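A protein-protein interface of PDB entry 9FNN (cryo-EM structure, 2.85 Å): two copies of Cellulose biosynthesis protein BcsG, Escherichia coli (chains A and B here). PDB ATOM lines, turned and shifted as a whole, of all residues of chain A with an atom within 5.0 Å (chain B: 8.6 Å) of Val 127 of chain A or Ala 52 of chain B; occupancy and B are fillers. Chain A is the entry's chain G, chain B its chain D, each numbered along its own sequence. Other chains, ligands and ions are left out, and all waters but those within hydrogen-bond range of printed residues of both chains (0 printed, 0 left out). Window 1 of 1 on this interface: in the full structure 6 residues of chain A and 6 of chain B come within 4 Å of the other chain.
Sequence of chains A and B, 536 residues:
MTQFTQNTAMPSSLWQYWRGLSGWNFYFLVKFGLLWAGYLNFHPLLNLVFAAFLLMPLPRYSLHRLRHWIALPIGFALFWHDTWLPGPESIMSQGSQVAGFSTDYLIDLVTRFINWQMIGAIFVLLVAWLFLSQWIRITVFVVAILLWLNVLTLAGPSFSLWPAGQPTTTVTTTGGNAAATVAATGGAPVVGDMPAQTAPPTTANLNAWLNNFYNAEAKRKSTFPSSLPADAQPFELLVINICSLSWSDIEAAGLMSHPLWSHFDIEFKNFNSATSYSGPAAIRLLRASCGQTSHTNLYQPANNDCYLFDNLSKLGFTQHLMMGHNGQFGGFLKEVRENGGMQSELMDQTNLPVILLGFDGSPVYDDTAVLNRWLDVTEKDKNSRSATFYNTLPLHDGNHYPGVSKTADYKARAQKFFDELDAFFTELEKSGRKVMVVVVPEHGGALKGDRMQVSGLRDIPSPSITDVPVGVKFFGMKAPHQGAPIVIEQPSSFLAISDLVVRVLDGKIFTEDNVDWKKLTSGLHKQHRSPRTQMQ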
ATOM      1  N   PHE A 123       0.691 -15.734  -9.042  1.00  0.00           N
ATOM      2  CA  PHE A 123       0.440 -16.829  -8.108  1.00  0.00           C
ATOM      3  C   PHE A 123       1.393 -16.777  -6.918  1.00  0.00           C
ATOM      4  O   PHE A 123       0.979 -16.973  -5.767  1.00  0.00           O
ATOM      5  CB  PHE A 123       0.558 -18.172  -8.827  1.00  0.00           C
ATOM      6  CG  PHE A 123       0.364 -19.358  -7.929  1.00  0.00           C
ATOM      7  CD1 PHE A 123      -0.902 -19.719  -7.503  1.00  0.00           C
ATOM      8  CD2 PHE A 123       1.446 -20.113  -7.513  1.00  0.00           C
ATOM      9  CE1 PHE A 123      -1.085 -20.810  -6.677  1.00  0.00           C
ATOM     10  CE2 PHE A 123       1.269 -21.205  -6.688  1.00  0.00           C
ATOM     11  CZ  PHE A 123       0.002 -21.552  -6.269  1.00  0.00           C
ATOM     12  N   VAL A 124       2.675 -16.510  -7.177  1.00  0.00           N
ATOM     13  CA  VAL A 124       3.647 -16.404  -6.092  1.00  0.00           C
ATOM     14  C   VAL A 124       3.305 -15.227  -5.187  1.00  0.00           C
ATOM     15  O   VAL A 124       3.436 -15.310  -3.961  1.00  0.00           O
ATOM     16  CB  VAL A 124       5.075 -16.295  -6.660  1.00  0.00           C
ATOM     17  CG1 VAL A 124       6.071 -15.999  -5.549  1.00  0.00           C
ATOM     18  CG2 VAL A 124       5.453 -17.578  -7.382  1.00  0.00           C
ATOM     19  N   LEU A 125       2.856 -14.116  -5.776  1.00  0.00           N
ATOM     20  CA  LEU A 125       2.466 -12.958  -4.978  1.00  0.00           C
ATOM     21  C   LEU A 125       1.236 -13.258  -4.131  1.00  0.00           C
ATOM     22  O   LEU A 125       1.139 -12.799  -2.990  1.00  0.00           O
ATOM     23  CB  LEU A 125       2.214 -11.755  -5.887  1.00  0.00           C
ATOM     24  CG  LEU A 125       3.429 -11.221  -6.646  1.00  0.00           C
ATOM     25  CD1 LEU A 125       3.012 -10.128  -7.618  1.00  0.00           C
ATOM     26  CD2 LEU A 125       4.486 -10.709  -5.680  1.00  0.00           C
ATOM     27  N   LEU A 126       0.282 -14.018  -4.672  1.00  0.00           N
ATOM     28  CA  LEU A 126      -0.884 -14.415  -3.889  1.00  0.00           C
ATOM     29  C   LEU A 126      -0.483 -15.298  -2.716  1.00  0.00           C
ATOM     30  O   LEU A 126      -0.981 -15.127  -1.596  1.00  0.00           O
ATOM     31  CB  LEU A 126      -1.897 -15.131  -4.784  1.00  0.00           C
ATOM     32  CG  LEU A 126      -3.191 -15.638  -4.141  1.00  0.00           C
ATOM     33  CD1 LEU A 126      -4.377 -15.362  -5.050  1.00  0.00           C
ATOM     34  CD2 LEU A 126      -3.099 -17.128  -3.831  1.00  0.00           C
ATOM     35  N   VAL A 127       0.420 -16.252  -2.955  1.00  0.00           N
ATOM     36  CA  VAL A 127       0.897 -17.109  -1.871  1.00  0.00           C
ATOM     37  C   VAL A 127       1.624 -16.279  -0.817  1.00  0.00           C
ATOM     38  O   VAL A 127       1.426 -16.467   0.391  1.00  0.00           O
ATOM     39  CB  VAL A 127       1.791 -18.229  -2.432  1.00  0.00           C
ATOM     40  CG1 VAL A 127       2.405 -19.039  -1.303  1.00  0.00           C
ATOM     41  CG2 VAL A 127       0.987 -19.128  -3.359  1.00  0.00           C
ATOM     42  N   ALA A 128       2.469 -15.344  -1.258  1.00  0.00           N
ATOM     43  CA  ALA A 128       3.208 -14.500  -0.328  1.00  0.00           C
ATOM     44  C   ALA A 128       2.289 -13.554   0.434  1.00  0.00           C
ATOM     45  O   ALA A 128       2.593 -13.190   1.571  1.00  0.00           O
ATOM     46  CB  ALA A 128       4.281 -13.708  -1.074  1.00  0.00           C
ATOM     47  N   TRP A 129       1.180 -13.133  -0.174  1.00  0.00           N
ATOM     48  CA  TRP A 129       0.223 -12.288   0.531  1.00  0.00           C
ATOM     49  C   TRP A 129      -0.571 -13.091   1.553  1.00  0.00           C
ATOM     50  O   TRP A 129      -0.864 -12.594   2.647  1.00  0.00           O
ATOM     51  CB  TRP A 129      -0.709 -11.607  -0.471  1.00  0.00           C
ATOM     52  CG  TRP A 129      -2.051 -11.251   0.091  1.00  0.00           C
ATOM     53  CD1 TRP A 129      -2.321 -10.312   1.043  1.00  0.00           C
ATOM     54  CD2 TRP A 129      -3.313 -11.824  -0.277  1.00  0.00           C
ATOM     55  NE1 TRP A 129      -3.671 -10.269   1.296  1.00  0.00           N
ATOM     56  CE2 TRP A 129      -4.302 -11.187   0.499  1.00  0.00           C
ATOM     57  CE3 TRP A 129      -3.700 -12.816  -1.183  1.00  0.00           C
ATOM     58  CZ2 TRP A 129      -5.654 -11.509   0.394  1.00  0.00           C
ATOM     59  CZ3 TRP A 129      -5.043 -13.134  -1.285  1.00  0.00           C
ATOM     60  CH2 TRP A 129      -6.003 -12.482  -0.502  1.00  0.00           C
ATOM     61  N   LEU A 130      -0.935 -14.329   1.212  1.00  0.00           N
ATOM     62  CA  LEU A 130      -1.623 -15.179   2.178  1.00  0.00           C
ATOM     63  C   LEU A 130      -0.709 -15.575   3.330  1.00  0.00           C
ATOM     64  O   LEU A 130      -1.186 -15.784   4.451  1.00  0.00           O
ATOM     65  CB  LEU A 130      -2.179 -16.425   1.488  1.00  0.00           C
ATOM     66  CG  LEU A 130      -3.512 -16.241   0.759  1.00  0.00           C
ATOM     67  CD1 LEU A 130      -3.973 -17.549   0.139  1.00  0.00           C
ATOM     68  CD2 LEU A 130      -4.567 -15.695   1.710  1.00  0.00           C
ATOM     69  N   PHE A 131       0.596 -15.684   3.081  1.00  0.00           N
ATOM     70  CA  PHE A 131       1.518 -16.003   4.165  1.00  0.00           C
ATOM     71  C   PHE A 131       1.855 -14.769   4.996  1.00  0.00           C
ATOM     72  O   PHE A 131       1.820 -14.814   6.230  1.00  0.00           O
ATOM     73  CB  PHE A 131       2.795 -16.634   3.608  1.00  0.00           C
ATOM     74  CG  PHE A 131       3.800 -16.995   4.667  1.00  0.00           C
ATOM     75  CD1 PHE A 131       3.639 -18.139   5.431  1.00  0.00           C
ATOM     76  CD2 PHE A 131       4.904 -16.189   4.898  1.00  0.00           C
ATOM     77  CE1 PHE A 131       4.559 -18.473   6.407  1.00  0.00           C
ATOM     78  CE2 PHE A 131       5.827 -16.519   5.872  1.00  0.00           C
ATOM     79  CZ  PHE A 131       5.655 -17.662   6.628  1.00  0.00           C
ATOM     80  N   LEU A 132       2.183 -13.657   4.336  1.00  0.00           N
ATOM     81  CA  LEU A 132       2.547 -12.428   5.028  1.00  0.00           C
ATOM     82  C   LEU A 132       1.355 -11.743   5.677  1.00  0.00           C
ATOM     83  O   LEU A 132       1.556 -10.817   6.466  1.00  0.00           O
ATOM     84  CB  LEU A 132       3.240 -11.464   4.064  1.00  0.00           C
ATOM     85  CG  LEU A 132       4.667 -11.840   3.659  1.00  0.00           C
ATOM     86  CD1 LEU A 132       5.271 -10.780   2.750  1.00  0.00           C
ATOM     87  CD2 LEU A 132       5.536 -12.054   4.890  1.00  0.00           C
ATOM     88  N   TRP B  18       0.155 -24.367   6.650  1.00  0.00           N
ATOM     89  CA  TRP B  18       1.510 -24.089   6.173  1.00  0.00           C
ATOM     90  C   TRP B  18       2.494 -25.000   6.907  1.00  0.00           C
ATOM     91  O   TRP B  18       3.313 -24.575   7.725  1.00  0.00           O
ATOM     92  CB  TRP B  18       1.849 -22.616   6.363  1.00  0.00           C
ATOM     93  CG  TRP B  18       0.987 -21.689   5.558  1.00  0.00           C
ATOM     94  CD1 TRP B  18      -0.292 -21.307   5.840  1.00  0.00           C
ATOM     95  CD2 TRP B  18       1.347 -21.020   4.343  1.00  0.00           C
ATOM     96  NE1 TRP B  18      -0.754 -20.448   4.873  1.00  0.00           N
ATOM     97  CE2 TRP B  18       0.233 -20.253   3.944  1.00  0.00           C
ATOM     98  CE3 TRP B  18       2.500 -20.995   3.553  1.00  0.00           C
ATOM     99  CZ2 TRP B  18       0.240 -19.472   2.791  1.00  0.00           C
ATOM    100  CZ3 TRP B  18       2.504 -20.218   2.408  1.00  0.00           C
ATOM    101  CH2 TRP B  18       1.380 -19.469   2.039  1.00  0.00           C
ATOM    102  N   LEU B  21       7.756 -27.352   3.470  1.00  0.00           N
ATOM    103  CA  LEU B  21       8.126 -28.147   2.304  1.00  0.00           C
ATOM    104  C   LEU B  21       8.336 -29.613   2.660  1.00  0.00           C
ATOM    105  O   LEU B  21       8.166 -30.485   1.800  1.00  0.00           O
ATOM    106  CB  LEU B  21       9.386 -27.573   1.656  1.00  0.00           C
ATOM    107  CG  LEU B  21       9.254 -26.167   1.070  1.00  0.00           C
ATOM    108  CD1 LEU B  21      10.592 -25.676   0.543  1.00  0.00           C
ATOM    109  CD2 LEU B  21       8.207 -26.148  -0.030  1.00  0.00           C
ATOM    110  N   PHE B  28      15.132 -29.353  -3.159  1.00  0.00           N
ATOM    111  CA  PHE B  28      15.631 -28.016  -3.458  1.00  0.00           C
ATOM    112  C   PHE B  28      17.115 -27.878  -3.138  1.00  0.00           C
ATOM    113  O   PHE B  28      17.837 -27.185  -3.861  1.00  0.00           O
ATOM    114  CB  PHE B  28      14.819 -26.965  -2.703  1.00  0.00           C
ATOM    115  CG  PHE B  28      13.503 -26.637  -3.352  1.00  0.00           C
ATOM    116  CD1 PHE B  28      13.456 -25.839  -4.484  1.00  0.00           C
ATOM    117  CD2 PHE B  28      12.314 -27.123  -2.833  1.00  0.00           C
ATOM    118  CE1 PHE B  28      12.248 -25.534  -5.087  1.00  0.00           C
ATOM    119  CE2 PHE B  28      11.104 -26.823  -3.431  1.00  0.00           C
ATOM    120  CZ  PHE B  28      11.071 -26.027  -4.559  1.00  0.00           C
ATOM    121  N   LEU B  45      12.136 -18.928 -11.896  1.00  0.00           N
ATOM    122  CA  LEU B  45      10.693 -18.707 -11.886  1.00  0.00           C
ATOM    123  C   LEU B  45       9.936 -20.017 -11.702  1.00  0.00           C
ATOM    124  O   LEU B  45       8.995 -20.094 -10.902  1.00  0.00           O
ATOM    125  CB  LEU B  45      10.262 -18.012 -13.177  1.00  0.00           C
ATOM    126  CG  LEU B  45       8.772 -17.694 -13.303  1.00  0.00           C
ATOM    127  CD1 LEU B  45       8.331 -16.738 -12.204  1.00  0.00           C
ATOM    128  CD2 LEU B  45       8.471 -17.118 -14.673  1.00  0.00           C
ATOM    129  N   LEU B  46      10.332 -21.059 -12.436  1.00  0.00           N
ATOM    130  CA  LEU B  46       9.669 -22.352 -12.305  1.00  0.00           C
ATOM    131  C   LEU B  46       9.878 -22.942 -10.917  1.00  0.00           C
ATOM    132  O   LEU B  46       8.948 -23.507 -10.331  1.00  0.00           O
ATOM    133  CB  LEU B  46      10.168 -23.313 -13.383  1.00  0.00           C
ATOM    134  CG  LEU B  46       9.378 -23.357 -14.693  1.00  0.00           C
ATOM    135  CD1 LEU B  46       7.928 -23.746 -14.430  1.00  0.00           C
ATOM    136  CD2 LEU B  46       9.453 -22.029 -15.436  1.00  0.00           C
ATOM    137  N   ASN B  47      11.092 -22.817 -10.375  1.00  0.00           N
ATOM    138  CA  ASN B  47      11.351 -23.302  -9.023  1.00  0.00           C
ATOM    139  C   ASN B  47      10.512 -22.555  -7.995  1.00  0.00           C
ATOM    140  O   ASN B  47       9.970 -23.164  -7.066  1.00  0.00           O
ATOM    141  CB  ASN B  47      12.839 -23.177  -8.695  1.00  0.00           C
ATOM    142  CG  ASN B  47      13.657 -24.321  -9.254  1.00  0.00           C
ATOM    143  OD1 ASN B  47      13.893 -25.318  -8.574  1.00  0.00           O
ATOM    144  ND2 ASN B  47      14.094 -24.184 -10.501  1.00  0.00           N
ATOM    145  N   LEU B  48      10.397 -21.233  -8.140  1.00  0.00           N
ATOM    146  CA  LEU B  48       9.594 -20.454  -7.203  1.00  0.00           C
ATOM    147  C   LEU B  48       8.118 -20.824  -7.297  1.00  0.00           C
ATOM    148  O   LEU B  48       7.433 -20.928  -6.272  1.00  0.00           O
ATOM    149  CB  LEU B  48       9.796 -18.961  -7.457  1.00  0.00           C
ATOM    150  CG  LEU B  48       9.224 -18.020  -6.397  1.00  0.00           C
ATOM    151  CD1 LEU B  48       9.762 -18.385  -5.023  1.00  0.00           C
ATOM    152  CD2 LEU B  48       9.548 -16.574  -6.735  1.00  0.00           C
ATOM    153  N   VAL B  49       7.612 -21.025  -8.515  1.00  0.00           N
ATOM    154  CA  VAL B  49       6.216 -21.426  -8.683  1.00  0.00           C
ATOM    155  C   VAL B  49       5.981 -22.802  -8.069  1.00  0.00           C
ATOM    156  O   VAL B  49       4.959 -23.038  -7.413  1.00  0.00           O
ATOM    157  CB  VAL B  49       5.823 -21.391 -10.172  1.00  0.00           C
ATOM    158  CG1 VAL B  49       4.460 -22.034 -10.381  1.00  0.00           C
ATOM    159  CG2 VAL B  49       5.812 -19.959 -10.680  1.00  0.00           C
ATOM    160  N   PHE B  50       6.921 -23.729  -8.270  1.00  0.00           N
ATOM    161  CA  PHE B  50       6.787 -25.058  -7.682  1.00  0.00           C
ATOM    162  C   PHE B  50       6.821 -24.995  -6.159  1.00  0.00           C
ATOM    163  O   PHE B  50       6.065 -25.703  -5.484  1.00  0.00           O
ATOM    164  CB  PHE B  50       7.890 -25.973  -8.216  1.00  0.00           C
ATOM    165  CG  PHE B  50       7.721 -27.414  -7.834  1.00  0.00           C
ATOM    166  CD1 PHE B  50       6.642 -28.145  -8.301  1.00  0.00           C
ATOM    167  CD2 PHE B  50       8.649 -28.041  -7.019  1.00  0.00           C
ATOM    168  CE1 PHE B  50       6.485 -29.473  -7.953  1.00  0.00           C
ATOM    169  CE2 PHE B  50       8.499 -29.369  -6.670  1.00  0.00           C
ATOM    170  CZ  PHE B  50       7.415 -30.086  -7.136  1.00  0.00           C
ATOM    171  N   ALA B  51       7.689 -24.150  -5.598  1.00  0.00           N
ATOM    172  CA  ALA B  51       7.739 -23.989  -4.148  1.00  0.00           C
ATOM    173  C   ALA B  51       6.442 -23.397  -3.610  1.00  0.00           C
ATOM    174  O   ALA B  51       5.948 -23.817  -2.558  1.00  0.00           O
ATOM    175  CB  ALA B  51       8.931 -23.117  -3.756  1.00  0.00           C
ATOM    176  N   ALA B  52       5.880 -22.411  -4.315  1.00  0.00           N
ATOM    177  CA  ALA B  52       4.600 -21.843  -3.905  1.00  0.00           C
ATOM    178  C   ALA B  52       3.490 -22.883  -3.977  1.00  0.00           C
ATOM    179  O   ALA B  52       2.598 -22.915  -3.121  1.00  0.00           O
ATOM    180  CB  ALA B  52       4.260 -20.631  -4.772  1.00  0.00           C
ATOM    181  N   PHE B  53       3.523 -23.737  -5.003  1.00  0.00           N
ATOM    182  CA  PHE B  53       2.557 -24.825  -5.105  1.00  0.00           C
ATOM    183  C   PHE B  53       2.700 -25.795  -3.938  1.00  0.00           C
ATOM    184  O   PHE B  53       1.701 -26.276  -3.391  1.00  0.00           O
ATOM    185  CB  PHE B  53       2.738 -25.549  -6.440  1.00  0.00           C
ATOM    186  CG  PHE B  53       1.618 -26.489  -6.785  1.00  0.00           C
ATOM    187  CD1 PHE B  53       0.466 -26.021  -7.391  1.00  0.00           C
ATOM    188  CD2 PHE B  53       1.725 -27.844  -6.518  1.00  0.00           C
ATOM    189  CE1 PHE B  53      -0.564 -26.882  -7.716  1.00  0.00           C
ATOM    190  CE2 PHE B  53       0.699 -28.711  -6.840  1.00  0.00           C
ATOM    191  CZ  PHE B  53      -0.448 -28.230  -7.439  1.00  0.00           C
ATOM    192  N   LEU B  54       3.941 -26.096  -3.548  1.00  0.00           N
ATOM    193  CA  LEU B  54       4.174 -26.991  -2.417  1.00  0.00           C
ATOM    194  C   LEU B  54       3.755 -26.362  -1.095  1.00  0.00           C
ATOM    195  O   LEU B  54       3.357 -27.079  -0.169  1.00  0.00           O
ATOM    196  CB  LEU B  54       5.647 -27.395  -2.360  1.00  0.00           C
ATOM    197  CG  LEU B  54       6.190 -28.239  -3.512  1.00  0.00           C
ATOM    198  CD1 LEU B  54       7.697 -28.376  -3.392  1.00  0.00           C
ATOM    199  CD2 LEU B  54       5.526 -29.607  -3.538  1.00  0.00           C
ATOM    200  N   LEU B  55       3.850 -25.039  -0.977  1.00  0.00           N
ATOM    201  CA  LEU B  55       3.502 -24.336   0.251  1.00  0.00           C
ATOM    202  C   LEU B  55       2.076 -23.799   0.247  1.00  0.00           C
ATOM    203  O   LEU B  55       1.699 -23.074   1.172  1.00  0.00           O
ATOM    204  CB  LEU B  55       4.486 -23.193   0.505  1.00  0.00           C
ATOM    205  CG  LEU B  55       5.831 -23.585   1.120  1.00  0.00           C
ATOM    206  CD1 LEU B  55       6.684 -22.354   1.376  1.00  0.00           C
ATOM    207  CD2 LEU B  55       5.619 -24.371   2.404  1.00  0.00           C
ATOM    208  N   MET B  56       1.285 -24.127  -0.765  1.00  0.00           N
ATOM    209  CA  MET B  56      -0.095 -23.658  -0.821  1.00  0.00           C
ATOM    210  C   MET B  56      -0.912 -24.317   0.283  1.00  0.00           C
ATOM    211  O   MET B  56      -0.968 -25.552   0.346  1.00  0.00           O
ATOM    212  CB  MET B  56      -0.703 -23.962  -2.187  1.00  0.00           C
ATOM    213  CG  MET B  56      -2.156 -23.535  -2.330  1.00  0.00           C
ATOM    214  SD  MET B  56      -2.374 -21.748  -2.214  1.00  0.00           S
ATOM    215  CE  MET B  56      -4.160 -21.621  -2.251  1.00  0.00           C
ATOM    216  N   PRO B  57      -1.552 -23.550   1.165  1.00  0.00           N
ATOM    217  CA  PRO B  57      -2.332 -24.167   2.245  1.00  0.00           C
ATOM    218  C   PRO B  57      -3.588 -24.841   1.716  1.00  0.00           C
ATOM    219  O   PRO B  57      -4.306 -24.292   0.876  1.00  0.00           O
ATOM    220  CB  PRO B  57      -2.672 -22.984   3.157  1.00  0.00           C
ATOM    221  CG  PRO B  57      -2.636 -21.798   2.255  1.00  0.00           C
ATOM    222  CD  PRO B  57      -1.554 -22.080   1.250  1.00  0.00           C
ATOM    223  N   ARG B  67      -2.140 -33.343  -3.517  1.00  0.00           N
ATOM    224  CA  ARG B  67      -1.248 -32.320  -4.045  1.00  0.00           C
ATOM    225  C   ARG B  67       0.190 -32.815  -4.086  1.00  0.00           C
ATOM    226  O   ARG B  67       0.904 -32.581  -5.067  1.00  0.00           O
ATOM    227  CB  ARG B  67      -1.353 -31.050  -3.202  1.00  0.00           C
ATOM    228  CG  ARG B  67      -0.598 -29.863  -3.767  1.00  0.00           C
ATOM    229  CD  ARG B  67      -0.392 -28.799  -2.708  1.00  0.00           C
ATOM    230  NE  ARG B  67       0.544 -29.242  -1.682  1.00  0.00           N
ATOM    231  CZ  ARG B  67       0.802 -28.578  -0.565  1.00  0.00           C
ATOM    232  NH1 ARG B  67       0.191 -27.440  -0.280  1.00  0.00           N
ATOM    233  NH2 ARG B  67       1.699 -29.066   0.287  1.00  0.00           N
ATOM    234  N   VAL B 143      12.996 -20.979   0.769  1.00  0.00           N
ATOM    235  CA  VAL B 143      12.210 -19.890   0.197  1.00  0.00           C
ATOM    236  C   VAL B 143      13.064 -18.638   0.043  1.00  0.00           C
ATOM    237  O   VAL B 143      12.999 -17.948  -0.983  1.00  0.00           O
ATOM    238  CB  VAL B 143      10.959 -19.625   1.055  1.00  0.00           C
ATOM    239  CG1 VAL B 143      10.250 -18.362   0.591  1.00  0.00           C
ATOM    240  CG2 VAL B 143      10.014 -20.813   0.989  1.00  0.00           C
ATOM    241  N   LEU B 146      15.471 -19.105  -2.900  1.00  0.00           N
ATOM    242  CA  LEU B 146      14.762 -19.000  -4.172  1.00  0.00           C
ATOM    243  C   LEU B 146      14.403 -17.553  -4.487  1.00  0.00           C
ATOM    244  O   LEU B 146      14.544 -17.107  -5.633  1.00  0.00           O
ATOM    245  CB  LEU B 146      13.512 -19.877  -4.147  1.00  0.00           C
ATOM    246  CG  LEU B 146      13.769 -21.384  -4.179  1.00  0.00           C
ATOM    247  CD1 LEU B 146      12.482 -22.150  -3.936  1.00  0.00           C
ATOM    248  CD2 LEU B 146      14.387 -21.782  -5.508  1.00  0.00           C
ATOM    249  N   LEU B 147      13.936 -16.803  -3.485  1.00  0.00           N
ATOM    250  CA  LEU B 147      13.624 -15.393  -3.699  1.00  0.00           C
ATOM    251  C   LEU B 147      14.871 -14.603  -4.074  1.00  0.00           C
ATOM    252  O   LEU B 147      14.825 -13.738  -4.956  1.00  0.00           O
ATOM    253  CB  LEU B 147      12.971 -14.799  -2.451  1.00  0.00           C
ATOM    254  CG  LEU B 147      11.444 -14.695  -2.438  1.00  0.00           C
ATOM    255  CD1 LEU B 147      10.951 -13.897  -3.637  1.00  0.00           C
ATOM    256  CD2 LEU B 147      10.795 -16.068  -2.398  1.00  0.00           C
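Among the printed residues, pairs that only touch across the chains: Val 127 of chain A with Trp 18 of chain B (3.4 Å), Phe 131 of chain A with Trp 18 of chain B (3.5 Å), Phe 123 of chain A with Ala 52 of chain B (3.6 Å), Val 124 of chain A with Leu 48 of chain B (3.7 Å), Phe 123 of chain A with Phe 53 of chain B (3.8 Å) and Val 127 of chain A with Ala 52 of chain B (3.9 Å).
Val 127 of chain A touches just these residues of chain B: Trp 18 (3.4 Å) and Ala 52 (3.9 Å). Of the printed residues of chain A, Ala 52 of chain B touches Phe 123 and Val 127. No residue of chain B comes within 4 Å of Ala 128 of chain A. Of the printed residues of chain A, Leu 48 of chain B touches Val 124. Of the printed residues of chain A, Phe 53 of chain B touches Phe 123. Printed residues of chain B within 4 Å of Phe 131 of chain A: Trp 18 (3.5 Å). The nearest residue of chain B that does not touch Val 127 of chain A is Met 56 of chain B (4.4 Å). The nearest residue of chain A that does not touch Ala 52 of chain B is Val 124 of chain A (4.2 Å).
Of the 10 printed residues of chain A, 4 touch a printed residue of chain B. Hydrophobic or aromatic side chains of chain B that line the printed part of chain A: Trp 18, Leu 48 and Ala 52. Among the printed residues, 6 pairs touch across the chains. Among the printed residues, no Asp or Glu carboxylate lies within 4 Å of a Lys or Arg side-chain nitrogen of the other chain.
No position is printed for both chains. Of the 6 pairs that touch across the chains among the printed residues, none has its exchanged pair printed and touching as well.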
